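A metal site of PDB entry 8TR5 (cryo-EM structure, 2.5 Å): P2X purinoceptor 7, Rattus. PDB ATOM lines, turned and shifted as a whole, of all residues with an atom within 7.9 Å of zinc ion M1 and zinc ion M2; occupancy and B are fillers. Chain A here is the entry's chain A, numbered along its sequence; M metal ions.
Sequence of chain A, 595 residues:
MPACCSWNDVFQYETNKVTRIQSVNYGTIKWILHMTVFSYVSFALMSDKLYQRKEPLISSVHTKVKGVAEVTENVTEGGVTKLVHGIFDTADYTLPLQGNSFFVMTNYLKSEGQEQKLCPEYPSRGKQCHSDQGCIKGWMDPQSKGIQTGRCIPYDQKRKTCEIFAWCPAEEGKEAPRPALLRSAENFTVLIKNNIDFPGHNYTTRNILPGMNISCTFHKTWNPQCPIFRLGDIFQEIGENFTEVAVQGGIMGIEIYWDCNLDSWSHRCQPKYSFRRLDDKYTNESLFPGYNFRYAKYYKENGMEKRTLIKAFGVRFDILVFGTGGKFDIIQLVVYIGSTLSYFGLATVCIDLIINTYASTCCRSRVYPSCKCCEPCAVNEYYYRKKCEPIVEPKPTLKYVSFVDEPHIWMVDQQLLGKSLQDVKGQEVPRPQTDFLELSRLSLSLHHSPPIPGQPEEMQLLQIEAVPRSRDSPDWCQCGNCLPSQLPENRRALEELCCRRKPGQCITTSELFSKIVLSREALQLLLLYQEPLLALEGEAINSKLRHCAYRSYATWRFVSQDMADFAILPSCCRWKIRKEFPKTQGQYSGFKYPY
Merely in contact with zinc ion M2: Gln 478 (3.9 Å). The nearest printed residue that does not touch zinc ion M2 is Gly 480 (4.01 Å).
The nearest printed residue that does not touch zinc ion M1 is Cys 482 (4.2 Å).
SG of Cys 572 binds zinc ion M1 (2.3 Å). SG of Cys 499 binds zinc ion M1, 2.3 Å away. The side-chain sulfur (SG) of Cys 506 is bound to zinc ion M1, 2.3 Å away. The side-chain sulfur (SG) of Cys 479 is bound to zinc ion M1, 2.3 Å away.
The backbone NH of Cys 572 sits close to the side-chain sulfur of Cys 482, 3.3 Å away. The side-chain sulfur (SG) of Cys 477 lies close to the backbone NH (N) of Gly 480 (3.0 Å). O of Cys 499 lies within hydrogen-bond range of N of Val 404, at 3.1 Å. The backbone carbonyl oxygen of Cys 506 lies within hydrogen-bond range of the side-chain hydroxyl of Thr 509 (2.6 Å). The side-chain sulfur of Cys 498 lies close to the backbone NH of Gln 478, at 3.2 Å. The backbone carbonyl oxygen (O) of Arg 500 sits close to the side-chain sulfur (SG) of Cys 498 (3.8 Å). The backbone NH (N) of Cys 498 is in hydrogen-bond range of the side-chain amide oxygen (OE1) of Gln 422, at 2.8 Å. The backbone NH (N) of Gly 504 lies within hydrogen-bond range of the backbone carbonyl oxygen (O) of Gln 478, at 3.2 Å.
Zinc ion M2 is bound by the side-chain sulfur (SG) of Cys 479, the side-chain sulfur (SG) of Cys 482, the side-chain sulfur (SG) of Cys 477 and the side-chain sulfur (SG) of Cys 498. Zinc ion M2 has four donor atoms within binding distance.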
ATOM      1  N   VAL A 404      20.867  29.563  27.368  1.00  0.00           N
ATOM      2  CA  VAL A 404      21.604  30.477  26.519  1.00  0.00           C
ATOM      3  C   VAL A 404      21.682  31.868  27.130  1.00  0.00           C
ATOM      4  O   VAL A 404      22.497  32.692  26.695  1.00  0.00           O
ATOM      5  CB  VAL A 404      20.985  30.509  25.118  1.00  0.00           C
ATOM      6  CG1 VAL A 404      19.609  31.103  25.167  1.00  0.00           C
ATOM      7  CG2 VAL A 404      21.858  31.297  24.182  1.00  0.00           C
ATOM      8  N   GLN A 422      12.876  22.481  34.215  1.00  0.00           N
ATOM      9  CA  GLN A 422      13.229  23.883  34.126  1.00  0.00           C
ATOM     10  C   GLN A 422      13.205  24.531  35.501  1.00  0.00           C
ATOM     11  O   GLN A 422      14.094  25.327  35.835  1.00  0.00           O
ATOM     12  CB  GLN A 422      12.259  24.588  33.184  1.00  0.00           C
ATOM     13  CG  GLN A 422      12.476  26.065  33.013  1.00  0.00           C
ATOM     14  CD  GLN A 422      13.477  26.388  31.941  1.00  0.00           C
ATOM     15  OE1 GLN A 422      14.085  25.505  31.358  1.00  0.00           O
ATOM     16  NE2 GLN A 422      13.635  27.665  31.667  1.00  0.00           N
ATOM     17  N   SER A 473       1.449  28.768  24.711  1.00  0.00           N
ATOM     18  CA  SER A 473       2.723  28.101  24.916  1.00  0.00           C
ATOM     19  C   SER A 473       2.843  27.617  26.361  1.00  0.00           C
ATOM     20  O   SER A 473       2.168  28.124  27.253  1.00  0.00           O
ATOM     21  CB  SER A 473       3.871  29.041  24.585  1.00  0.00           C
ATOM     22  OG  SER A 473       5.047  28.675  25.279  1.00  0.00           O
ATOM     23  N   PRO A 474       3.694  26.619  26.608  1.00  0.00           N
ATOM     24  CA  PRO A 474       3.844  26.104  27.963  1.00  0.00           C
ATOM     25  C   PRO A 474       4.295  27.170  28.942  1.00  0.00           C
ATOM     26  O   PRO A 474       5.027  28.095  28.593  1.00  0.00           O
ATOM     27  CB  PRO A 474       4.893  25.007  27.818  1.00  0.00           C
ATOM     28  CG  PRO A 474       4.809  24.595  26.412  1.00  0.00           C
ATOM     29  CD  PRO A 474       4.437  25.806  25.634  1.00  0.00           C
ATOM     30  N   TRP A 476       6.295  26.882  31.534  1.00  0.00           N
ATOM     31  CA  TRP A 476       7.727  26.804  31.777  1.00  0.00           C
ATOM     32  C   TRP A 476       8.555  27.296  30.601  1.00  0.00           C
ATOM     33  O   TRP A 476       9.776  27.438  30.746  1.00  0.00           O
ATOM     34  CB  TRP A 476       8.132  25.376  32.123  1.00  0.00           C
ATOM     35  CG  TRP A 476       7.556  24.335  31.227  1.00  0.00           C
ATOM     36  CD1 TRP A 476       6.442  23.595  31.458  1.00  0.00           C
ATOM     37  CD2 TRP A 476       8.048  23.920  29.959  1.00  0.00           C
ATOM     38  NE1 TRP A 476       6.201  22.748  30.413  1.00  0.00           N
ATOM     39  CE2 TRP A 476       7.180  22.930  29.476  1.00  0.00           C
ATOM     40  CE3 TRP A 476       9.146  24.299  29.180  1.00  0.00           C
ATOM     41  CZ2 TRP A 476       7.376  22.302  28.258  1.00  0.00           C
ATOM     42  CZ3 TRP A 476       9.326  23.682  27.975  1.00  0.00           C
ATOM     43  CH2 TRP A 476       8.451  22.695  27.520  1.00  0.00           C
ATOM     44  N   CYS A 477       7.937  27.555  29.451  1.00  0.00           N
ATOM     45  CA  CYS A 477       8.680  28.020  28.291  1.00  0.00           C
ATOM     46  C   CYS A 477       8.815  29.531  28.331  1.00  0.00           C
ATOM     47  O   CYS A 477       7.824  30.253  28.475  1.00  0.00           O
ATOM     48  CB  CYS A 477       7.987  27.597  26.996  1.00  0.00           C
ATOM     49  SG  CYS A 477       8.705  28.347  25.538  1.00  0.00           S
ATOM     50  N   GLN A 478      10.045  30.007  28.173  1.00  0.00           N
ATOM     51  CA  GLN A 478      10.349  31.425  28.138  1.00  0.00           C
ATOM     52  C   GLN A 478      10.844  31.867  26.758  1.00  0.00           C
ATOM     53  O   GLN A 478      11.507  32.894  26.634  1.00  0.00           O
ATOM     54  CB  GLN A 478      11.379  31.774  29.203  1.00  0.00           C
ATOM     55  CG  GLN A 478      11.197  31.044  30.516  1.00  0.00           C
ATOM     56  CD  GLN A 478      10.163  31.678  31.409  1.00  0.00           C
ATOM     57  OE1 GLN A 478       9.234  32.340  30.931  1.00  0.00           O
ATOM     58  NE2 GLN A 478      10.294  31.464  32.699  1.00  0.00           N
ATOM     59  N   CYS A 479      10.536  31.087  25.727  1.00  0.00           N
ATOM     60  CA  CYS A 479      10.964  31.386  24.371  1.00  0.00           C
ATOM     61  C   CYS A 479       9.866  31.297  23.329  1.00  0.00           C
ATOM     62  O   CYS A 479      10.025  31.855  22.245  1.00  0.00           O
ATOM     63  CB  CYS A 479      12.117  30.442  23.962  1.00  0.00           C
ATOM     64  SG  CYS A 479      11.627  28.807  23.356  1.00  0.00           S
ATOM     65  N   GLY A 480       8.747  30.622  23.629  1.00  0.00           N
ATOM     66  CA  GLY A 480       7.631  30.555  22.726  1.00  0.00           C
ATOM     67  C   GLY A 480       7.662  29.410  21.736  1.00  0.00           C
ATOM     68  O   GLY A 480       6.629  29.121  21.121  1.00  0.00           O
ATOM     69  N   ASN A 481       8.796  28.744  21.575  1.00  0.00           N
ATOM     70  CA  ASN A 481       8.945  27.681  20.605  1.00  0.00           C
ATOM     71  C   ASN A 481       8.865  26.289  21.208  1.00  0.00           C
ATOM     72  O   ASN A 481       8.830  25.306  20.459  1.00  0.00           O
ATOM     73  CB  ASN A 481      10.276  27.824  19.858  1.00  0.00           C
ATOM     74  CG  ASN A 481      10.244  28.918  18.817  1.00  0.00           C
ATOM     75  OD1 ASN A 481      10.780  30.015  19.026  1.00  0.00           O
ATOM     76  ND2 ASN A 481       9.613  28.641  17.684  1.00  0.00           N
ATOM     77  N   CYS A 482       8.816  26.178  22.524  1.00  0.00           N
ATOM     78  CA  CYS A 482       8.763  24.873  23.168  1.00  0.00           C
ATOM     79  C   CYS A 482       7.352  24.311  23.117  1.00  0.00           C
ATOM     80  O   CYS A 482       6.362  25.045  23.040  1.00  0.00           O
ATOM     81  CB  CYS A 482       9.252  24.962  24.604  1.00  0.00           C
ATOM     82  SG  CYS A 482      10.994  25.338  24.784  1.00  0.00           S
ATOM     83  N   LEU A 483       7.264  22.990  23.182  1.00  0.00           N
ATOM     84  CA  LEU A 483       6.020  22.261  23.046  1.00  0.00           C
ATOM     85  C   LEU A 483       5.890  21.244  24.175  1.00  0.00           C
ATOM     86  O   LEU A 483       6.893  20.845  24.778  1.00  0.00           O
ATOM     87  CB  LEU A 483       5.950  21.530  21.699  1.00  0.00           C
ATOM     88  CG  LEU A 483       6.080  22.412  20.458  1.00  0.00           C
ATOM     89  CD1 LEU A 483       6.238  21.623  19.169  1.00  0.00           C
ATOM     90  CD2 LEU A 483       5.083  23.566  20.342  1.00  0.00           C
ATOM     91  N   LEU A 497      11.729  21.435  29.534  1.00  0.00           N
ATOM     92  CA  LEU A 497      12.875  22.308  29.676  1.00  0.00           C
ATOM     93  C   LEU A 497      12.929  23.280  28.514  1.00  0.00           C
ATOM     94  O   LEU A 497      12.676  22.897  27.370  1.00  0.00           O
ATOM     95  CB  LEU A 497      14.164  21.494  29.757  1.00  0.00           C
ATOM     96  CG  LEU A 497      15.486  22.225  29.893  1.00  0.00           C
ATOM     97  CD1 LEU A 497      15.731  22.635  31.307  1.00  0.00           C
ATOM     98  CD2 LEU A 497      16.568  21.319  29.427  1.00  0.00           C
ATOM     99  N   CYS A 498      13.274  24.527  28.811  1.00  0.00           N
ATOM    100  CA  CYS A 498      13.361  25.575  27.813  1.00  0.00           C
ATOM    101  C   CYS A 498      14.810  25.913  27.512  1.00  0.00           C
ATOM    102  O   CYS A 498      15.730  25.566  28.250  1.00  0.00           O
ATOM    103  CB  CYS A 498      12.635  26.835  28.281  1.00  0.00           C
ATOM    104  SG  CYS A 498      12.311  28.046  27.000  1.00  0.00           S
ATOM    105  N   CYS A 499      15.010  26.614  26.393  1.00  0.00           N
ATOM    106  CA  CYS A 499      16.346  27.029  25.988  1.00  0.00           C
ATOM    107  C   CYS A 499      16.905  28.116  26.890  1.00  0.00           C
ATOM    108  O   CYS A 499      18.130  28.217  27.026  1.00  0.00           O
ATOM    109  CB  CYS A 499      16.329  27.518  24.546  1.00  0.00           C
ATOM    110  SG  CYS A 499      15.248  28.896  24.227  1.00  0.00           S
ATOM    111  N   ARG A 500      16.048  28.921  27.505  1.00  0.00           N
ATOM    112  CA  ARG A 500      16.493  30.020  28.334  1.00  0.00           C
ATOM    113  C   ARG A 500      15.671  30.072  29.608  1.00  0.00           C
ATOM    114  O   ARG A 500      14.520  29.615  29.654  1.00  0.00           O
ATOM    115  CB  ARG A 500      16.403  31.359  27.605  1.00  0.00           C
ATOM    116  CG  ARG A 500      15.101  31.593  26.883  1.00  0.00           C
ATOM    117  CD  ARG A 500      15.202  32.839  26.057  1.00  0.00           C
ATOM    118  NE  ARG A 500      15.903  33.887  26.778  1.00  0.00           N
ATOM    119  CZ  ARG A 500      16.902  34.624  26.299  1.00  0.00           C
ATOM    120  NH1 ARG A 500      17.340  34.452  25.063  1.00  0.00           N
ATOM    121  NH2 ARG A 500      17.460  35.538  27.072  1.00  0.00           N
ATOM    122  N   GLY A 504      12.988  35.744  26.246  1.00  0.00           N
ATOM    123  CA  GLY A 504      13.887  36.208  25.216  1.00  0.00           C
ATOM    124  C   GLY A 504      13.692  35.408  23.943  1.00  0.00           C
ATOM    125  O   GLY A 504      12.683  34.715  23.775  1.00  0.00           O
ATOM    126  N   GLN A 505      14.672  35.514  23.066  1.00  0.00           N
ATOM    127  CA  GLN A 505      14.607  34.811  21.791  1.00  0.00           C
ATOM    128  C   GLN A 505      15.124  33.391  21.934  1.00  0.00           C
ATOM    129  O   GLN A 505      16.053  33.118  22.703  1.00  0.00           O
ATOM    130  CB  GLN A 505      15.412  35.564  20.726  1.00  0.00           C
ATOM    131  CG  GLN A 505      16.795  35.985  21.167  1.00  0.00           C
ATOM    132  CD  GLN A 505      17.686  36.358  20.002  1.00  0.00           C
ATOM    133  OE1 GLN A 505      17.480  35.902  18.873  1.00  0.00           O
ATOM    134  NE2 GLN A 505      18.676  37.185  20.267  1.00  0.00           N
ATOM    135  N   CYS A 506      14.512  32.481  21.188  1.00  0.00           N
ATOM    136  CA  CYS A 506      14.919  31.085  21.225  1.00  0.00           C
ATOM    137  C   CYS A 506      16.279  30.906  20.564  1.00  0.00           C
ATOM    138  O   CYS A 506      16.640  31.605  19.609  1.00  0.00           O
ATOM    139  CB  CYS A 506      13.877  30.215  20.531  1.00  0.00           C
ATOM    140  SG  CYS A 506      14.214  28.462  20.576  1.00  0.00           S
ATOM    141  N   ILE A 507      17.037  29.945  21.087  1.00  0.00           N
ATOM    142  CA  ILE A 507      18.343  29.615  20.524  1.00  0.00           C
ATOM    143  C   ILE A 507      18.186  29.097  19.103  1.00  0.00           C
ATOM    144  O   ILE A 507      19.134  29.174  18.300  1.00  0.00           O
ATOM    145  CB  ILE A 507      19.057  28.608  21.431  1.00  0.00           C
ATOM    146  CG1 ILE A 507      20.521  28.498  21.055  1.00  0.00           C
ATOM    147  CG2 ILE A 507      18.404  27.268  21.318  1.00  0.00           C
ATOM    148  CD1 ILE A 507      21.300  27.657  21.998  1.00  0.00           C
ATOM    149  N   THR A 508      17.019  28.568  18.774  1.00  0.00           N
ATOM    150  CA  THR A 508      16.764  28.095  17.419  1.00  0.00           C
ATOM    151  C   THR A 508      16.831  29.214  16.392  1.00  0.00           C
ATOM    152  O   THR A 508      17.017  28.948  15.206  1.00  0.00           O
ATOM    153  CB  THR A 508      15.401  27.430  17.346  1.00  0.00           C
ATOM    154  OG1 THR A 508      14.387  28.336  17.792  1.00  0.00           O
ATOM    155  CG2 THR A 508      15.376  26.206  18.207  1.00  0.00           C
ATOM    156  N   THR A 509      16.671  30.469  16.822  1.00  0.00           N
ATOM    157  CA  THR A 509      16.760  31.587  15.904  1.00  0.00           C
ATOM    158  C   THR A 509      18.192  31.856  15.470  1.00  0.00           C
ATOM    159  O   THR A 509      18.408  32.501  14.437  1.00  0.00           O
ATOM    160  CB  THR A 509      16.167  32.838  16.546  1.00  0.00           C
ATOM    161  OG1 THR A 509      16.966  33.232  17.657  1.00  0.00           O
ATOM    162  CG2 THR A 509      14.750  32.554  17.014  1.00  0.00           C
ATOM    163  N   PRO A 570      16.520  21.129  25.154  1.00  0.00           N
ATOM    164  CA  PRO A 570      15.256  21.843  25.338  1.00  0.00           C
ATOM    165  C   PRO A 570      14.174  21.324  24.421  1.00  0.00           C
ATOM    166  O   PRO A 570      14.447  20.726  23.373  1.00  0.00           O
ATOM    167  CB  PRO A 570      15.627  23.292  25.010  1.00  0.00           C
ATOM    168  CG  PRO A 570      17.054  23.366  25.195  1.00  0.00           C
ATOM    169  CD  PRO A 570      17.604  22.058  24.810  1.00  0.00           C
ATOM    170  N   SER A 571      12.932  21.543  24.818  1.00  0.00           N
ATOM    171  CA  SER A 571      11.814  21.110  23.994  1.00  0.00           C
ATOM    172  C   SER A 571      11.808  21.813  22.648  1.00  0.00           C
ATOM    173  O   SER A 571      11.499  21.205  21.628  1.00  0.00           O
ATOM    174  CB  SER A 571      10.498  21.360  24.728  1.00  0.00           C
ATOM    175  OG  SER A 571       9.476  20.487  24.276  1.00  0.00           O
ATOM    176  N   CYS A 572      12.167  23.100  22.634  1.00  0.00           N
ATOM    177  CA  CYS A 572      12.179  23.842  21.382  1.00  0.00           C
ATOM    178  C   CYS A 572      13.171  23.252  20.398  1.00  0.00           C
ATOM    179  O   CYS A 572      12.811  22.940  19.253  1.00  0.00           O
ATOM    180  CB  CYS A 572      12.500  25.308  21.662  1.00  0.00           C
ATOM    181  SG  CYS A 572      13.852  25.585  22.819  1.00  0.00           S
ATOM    182  N   CYS A 573      14.414  23.062  20.819  1.00  0.00           N
ATOM    183  CA  CYS A 573      15.430  22.515  19.941  1.00  0.00           C
ATOM    184  C   CYS A 573      15.120  21.067  19.568  1.00  0.00           C
ATOM    185  O   CYS A 573      15.273  20.671  18.407  1.00  0.00           O
ATOM    186  CB  CYS A 573      16.795  22.629  20.618  1.00  0.00           C
ATOM    187  SG  CYS A 573      17.094  24.249  21.317  1.00  0.00           S
HETATM  188 ZN    ZN M   1      13.712  27.906  22.782  1.00  0.00          ZN
HETATM  189 ZN    ZN M   2      10.892  27.619  25.204  1.00  0.00          ZN
